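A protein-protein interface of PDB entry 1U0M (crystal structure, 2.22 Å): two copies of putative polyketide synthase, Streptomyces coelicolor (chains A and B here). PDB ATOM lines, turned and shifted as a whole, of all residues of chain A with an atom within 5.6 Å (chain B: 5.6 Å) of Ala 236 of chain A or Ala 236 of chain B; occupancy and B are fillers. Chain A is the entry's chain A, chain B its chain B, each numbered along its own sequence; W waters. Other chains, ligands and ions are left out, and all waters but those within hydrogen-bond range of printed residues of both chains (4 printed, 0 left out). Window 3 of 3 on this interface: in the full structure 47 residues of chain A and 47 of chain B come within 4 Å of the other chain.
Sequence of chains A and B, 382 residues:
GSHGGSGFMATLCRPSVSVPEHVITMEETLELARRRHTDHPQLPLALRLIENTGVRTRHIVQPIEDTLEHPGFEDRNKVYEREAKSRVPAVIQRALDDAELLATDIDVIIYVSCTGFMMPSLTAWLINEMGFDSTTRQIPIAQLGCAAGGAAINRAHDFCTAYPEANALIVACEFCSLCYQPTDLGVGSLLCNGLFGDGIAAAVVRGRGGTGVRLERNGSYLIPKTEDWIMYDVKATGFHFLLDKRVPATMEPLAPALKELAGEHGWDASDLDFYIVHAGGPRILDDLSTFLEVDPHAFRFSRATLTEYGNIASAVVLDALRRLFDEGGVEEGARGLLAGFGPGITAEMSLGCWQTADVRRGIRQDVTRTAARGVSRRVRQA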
ATOM      1  N   PHE A  73      12.559 -22.604  29.843  1.00  0.00           N
ATOM      2  CA  PHE A  73      11.950 -21.323  29.464  1.00  0.00           C
ATOM      3  C   PHE A  73      10.785 -21.520  28.482  1.00  0.00           C
ATOM      4  O   PHE A  73       9.769 -20.827  28.567  1.00  0.00           O
ATOM      5  CB  PHE A  73      13.048 -20.436  28.848  1.00  0.00           C
ATOM      6  CG  PHE A  73      12.614 -19.037  28.518  1.00  0.00           C
ATOM      7  CD1 PHE A  73      13.241 -18.341  27.482  1.00  0.00           C
ATOM      8  CD2 PHE A  73      11.613 -18.400  29.239  1.00  0.00           C
ATOM      9  CE1 PHE A  73      12.881 -17.040  27.171  1.00  0.00           C
ATOM     10  CE2 PHE A  73      11.244 -17.099  28.931  1.00  0.00           C
ATOM     11  CZ  PHE A  73      11.880 -16.415  27.895  1.00  0.00           C
ATOM     12  N   GLU A  74      10.929 -22.462  27.547  1.00  0.00           N
ATOM     13  CA  GLU A  74       9.866 -22.728  26.572  1.00  0.00           C
ATOM     14  C   GLU A  74       8.593 -23.184  27.292  1.00  0.00           C
ATOM     15  O   GLU A  74       7.521 -22.631  27.063  1.00  0.00           O
ATOM     16  CB  GLU A  74      10.305 -23.787  25.545  1.00  0.00           C
ATOM     17  CG  GLU A  74       9.175 -24.225  24.602  1.00  0.00           C
ATOM     18  CD  GLU A  74       9.635 -25.062  23.405  1.00  0.00           C
ATOM     19  OE1 GLU A  74      10.746 -25.638  23.448  1.00  0.00           O
ATOM     20  OE2 GLU A  74       8.857 -25.156  22.421  1.00  0.00           O
ATOM     21  N   VAL A 234      19.348 -12.069  30.525  1.00  0.00           N
ATOM     22  CA  VAL A 234      18.563 -12.955  29.655  1.00  0.00           C
ATOM     23  C   VAL A 234      19.360 -14.174  29.203  1.00  0.00           C
ATOM     24  O   VAL A 234      20.263 -14.071  28.372  1.00  0.00           O
ATOM     25  CB  VAL A 234      18.058 -12.202  28.417  1.00  0.00           C
ATOM     26  CG1 VAL A 234      17.238 -13.142  27.533  1.00  0.00           C
ATOM     27  CG2 VAL A 234      17.218 -10.990  28.860  1.00  0.00           C
ATOM     28  N   LYS A 235      18.991 -15.334  29.735  1.00  0.00           N
ATOM     29  CA  LYS A 235      19.687 -16.582  29.447  1.00  0.00           C
ATOM     30  C   LYS A 235      18.805 -17.658  28.823  1.00  0.00           C
ATOM     31  O   LYS A 235      17.609 -17.473  28.624  1.00  0.00           O
ATOM     32  CB  LYS A 235      20.268 -17.130  30.750  1.00  0.00           C
ATOM     33  CG  LYS A 235      21.179 -16.151  31.459  1.00  0.00           C
ATOM     34  CD  LYS A 235      21.529 -16.608  32.846  1.00  0.00           C
ATOM     35  CE  LYS A 235      22.486 -15.615  33.505  1.00  0.00           C
ATOM     36  NZ  LYS A 235      23.008 -16.169  34.766  1.00  0.00           N
ATOM     37  N   ALA A 236      19.411 -18.808  28.553  1.00  0.00           N
ATOM     38  CA  ALA A 236      18.683 -19.922  27.986  1.00  0.00           C
ATOM     39  C   ALA A 236      17.605 -20.371  28.974  1.00  0.00           C
ATOM     40  O   ALA A 236      16.619 -20.980  28.582  1.00  0.00           O
ATOM     41  CB  ALA A 236      19.638 -21.055  27.703  1.00  0.00           C
ATOM     42  N   THR A 237      17.807 -20.065  30.258  1.00  0.00           N
ATOM     43  CA  THR A 237      16.866 -20.438  31.315  1.00  0.00           C
ATOM     44  C   THR A 237      15.759 -19.404  31.476  1.00  0.00           C
ATOM     45  O   THR A 237      14.809 -19.584  32.249  1.00  0.00           O
ATOM     46  CB  THR A 237      17.593 -20.595  32.666  1.00  0.00           C
ATOM     47  OG1 THR A 237      18.730 -19.735  32.686  1.00  0.00           O
ATOM     48  CG2 THR A 237      18.052 -22.026  32.879  1.00  0.00           C
ATOM     49  N   GLY A 238      15.885 -18.301  30.754  1.00  0.00           N
ATOM     50  CA  GLY A 238      14.866 -17.282  30.834  1.00  0.00           C
ATOM     51  C   GLY A 238      15.375 -15.981  31.394  1.00  0.00           C
ATOM     52  O   GLY A 238      16.521 -15.602  31.162  1.00  0.00           O
ATOM     53  N   PHE B  73      21.362 -18.453  23.432  1.00  0.00           N
ATOM     54  CA  PHE B  73      20.563 -17.233  23.571  1.00  0.00           C
ATOM     55  C   PHE B  73      21.304 -16.205  24.450  1.00  0.00           C
ATOM     56  O   PHE B  73      21.394 -15.034  24.088  1.00  0.00           O
ATOM     57  CB  PHE B  73      19.196 -17.613  24.183  1.00  0.00           C
ATOM     58  CG  PHE B  73      18.175 -16.499  24.196  1.00  0.00           C
ATOM     59  CD1 PHE B  73      17.118 -16.540  25.106  1.00  0.00           C
ATOM     60  CD2 PHE B  73      18.245 -15.434  23.296  1.00  0.00           C
ATOM     61  CE1 PHE B  73      16.146 -15.543  25.125  1.00  0.00           C
ATOM     62  CE2 PHE B  73      17.285 -14.432  23.301  1.00  0.00           C
ATOM     63  CZ  PHE B  73      16.220 -14.489  24.231  1.00  0.00           C
ATOM     64  N   GLU B  74      21.846 -16.636  25.591  1.00  0.00           N
ATOM     65  CA  GLU B  74      22.570 -15.710  26.479  1.00  0.00           C
ATOM     66  C   GLU B  74      23.632 -14.948  25.673  1.00  0.00           C
ATOM     67  O   GLU B  74      23.599 -13.714  25.602  1.00  0.00           O
ATOM     68  CB  GLU B  74      23.233 -16.464  27.650  1.00  0.00           C
ATOM     69  CG  GLU B  74      23.797 -15.538  28.755  1.00  0.00           C
ATOM     70  CD  GLU B  74      24.440 -16.279  29.933  1.00  0.00           C
ATOM     71  OE1 GLU B  74      24.081 -17.445  30.202  1.00  0.00           O
ATOM     72  OE2 GLU B  74      25.303 -15.680  30.607  1.00  0.00           O
ATOM     73  N   VAL B 234       8.971 -18.985  21.575  1.00  0.00           N
ATOM     74  CA  VAL B 234      10.009 -18.618  22.544  1.00  0.00           C
ATOM     75  C   VAL B 234      10.599 -19.845  23.237  1.00  0.00           C
ATOM     76  O   VAL B 234       9.936 -20.481  24.053  1.00  0.00           O
ATOM     77  CB  VAL B 234       9.440 -17.659  23.606  1.00  0.00           C
ATOM     78  CG1 VAL B 234      10.515 -17.317  24.644  1.00  0.00           C
ATOM     79  CG2 VAL B 234       8.940 -16.389  22.922  1.00  0.00           C
ATOM     80  N   LYS B 235      11.855 -20.156  22.930  1.00  0.00           N
ATOM     81  CA  LYS B 235      12.512 -21.336  23.486  1.00  0.00           C
ATOM     82  C   LYS B 235      13.835 -21.028  24.183  1.00  0.00           C
ATOM     83  O   LYS B 235      14.285 -19.891  24.209  1.00  0.00           O
ATOM     84  CB  LYS B 235      12.778 -22.337  22.348  1.00  0.00           C
ATOM     85  CG  LYS B 235      11.556 -22.598  21.488  1.00  0.00           C
ATOM     86  CD  LYS B 235      11.873 -23.462  20.296  1.00  0.00           C
ATOM     87  CE  LYS B 235      10.584 -23.984  19.661  1.00  0.00           C
ATOM     88  NZ  LYS B 235      10.875 -24.774  18.449  1.00  0.00           N
ATOM     89  N   ALA B 236      14.465 -22.072  24.716  1.00  0.00           N
ATOM     90  CA  ALA B 236      15.753 -21.944  25.390  1.00  0.00           C
ATOM     91  C   ALA B 236      16.819 -21.426  24.426  1.00  0.00           C
ATOM     92  O   ALA B 236      17.867 -20.957  24.848  1.00  0.00           O
ATOM     93  CB  ALA B 236      16.178 -23.284  25.957  1.00  0.00           C
ATOM     94  N   THR B 237      16.541 -21.508  23.128  1.00  0.00           N
ATOM     95  CA  THR B 237      17.469 -21.028  22.123  1.00  0.00           C
ATOM     96  C   THR B 237      17.140 -19.598  21.694  1.00  0.00           C
ATOM     97  O   THR B 237      17.878 -18.967  20.933  1.00  0.00           O
ATOM     98  CB  THR B 237      17.458 -21.956  20.903  1.00  0.00           C
ATOM     99  OG1 THR B 237      16.126 -22.418  20.676  1.00  0.00           O
ATOM    100  CG2 THR B 237      18.353 -23.175  21.149  1.00  0.00           C
ATOM    101  N   GLY B 238      16.030 -19.070  22.184  1.00  0.00           N
ATOM    102  CA  GLY B 238      15.686 -17.707  21.816  1.00  0.00           C
ATOM    103  C   GLY B 238      14.378 -17.593  21.057  1.00  0.00           C
ATOM    104  O   GLY B 238      13.397 -18.266  21.385  1.00  0.00           O
HETATM  105  O   HOH W   1      13.089 -24.856  24.411  1.00  0.00           O
HETATM  106  O   HOH W   2       7.134 -20.930  24.805  1.00  0.00           O
HETATM  107  O   HOH W   3      22.100 -11.588  27.559  1.00  0.00           O
HETATM  108  O   HOH W   4      22.439 -19.276  29.160  1.00  0.00           O
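Ala 236 of chain A touches one residue of chain B. Ala 236 of chain B touches just one residue of chain A: Ala 236 (3.4 Å). Printed residues of chain A within 4 Å of Lys 235 of chain B: Phe 73 (3.8 Å) and Glu 74 (3.5 Å). Printed residues of chain B within 4 Å of Glu 74 of chain A: Val 234 and Lys 235. Of the printed residues of chain A, Glu 74 of chain B touches Val 234 and Lys 235. Of the printed residues of chain A, Val 234 of chain B touches Phe 73 and Glu 74. Thr 237 of chain A touches none of the printed residues of chain B. The nearest residue of chain B that does not touch Ala 236 of chain A is Glu 74 of chain B (4.4 Å). The nearest residue of chain A that does not touch Ala 236 of chain B is Glu 74 of chain A (4.5 Å). The nearest printed residue of chain B that does not touch Val 234 of chain A is Gly 238 of chain B (7.5 Å).
Of the 7 printed residues of chain A, 5 touch a printed residue of chain B. Of the 7 printed residues of chain B, 5 touch a printed residue of chain A. Hydrophobic or aromatic side chains of chain B within 4 Å of the printed part of chain A: Phe 73, Val 234 and Ala 236. Among the printed residues, no Asp or Glu carboxylate lies within 4 Å of a Lys or Arg side-chain nitrogen of the other chain.
Phe 73 of chain A touches Val 234 of chain B, and with the chains exchanged Val 234 of chain A touches Phe 73 of chain B. Glu 74 of chain A touches Val 234 of chain B, and with the chains exchanged Val 234 of chain A touches Glu 74 of chain B. Glu 74 of chain A touches Lys 235 of chain B, and with the chains exchanged Lys 235 of chain A touches Glu 74 of chain B. Ala 236 of chain B touches its own counterpart, Ala 236 of chain A. Positions printed for both chains: 73, 74, 234, 235, 236, 237 and 238. Of the 9 pairs that touch across the chains among the printed residues, 9 have their exchanged pair printed and touching as well.
Water W1 lies within hydrogen-bond range of the side-chain carboxylate of Glu 74 of chain A (2.7 Å) and the backbone NH of Ala 236 of chain B (3.1 Å). Water W4 lies within hydrogen-bond range of the side-chain carboxylate of Glu 74 of chain B and the backbone NH of Ala 236 of chain A. Water W2 bridges O of Glu 74 of chain A (2.9 Å) and O of Val 234 of chain B (2.9 Å). Water W3 lies within hydrogen-bond range of the backbone carbonyl oxygen (O) of Val 234 of chain A (3.2 Å) and the backbone carbonyl oxygen (O) of Glu 74 of chain B (3.3 Å).
Among the printed residues, merely in contact across the chains: Ala 236 of chain A with Ala 236 of chain B, Glu 74 of chain A with Val 234 of chain B, Val 234 of chain A with Glu 74 of chain B, Lys 235 of chain A with Glu 74 of chain B, Glu 74 of chain A with Lys 235 of chain B, Phe 73 of chain A with Val 234 of chain B, Val 234 of chain A with Phe 73 of chain B, Lys 235 of chain A with Phe 73 of chain B and Phe 73 of chain A with Lys 235 of chain B.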
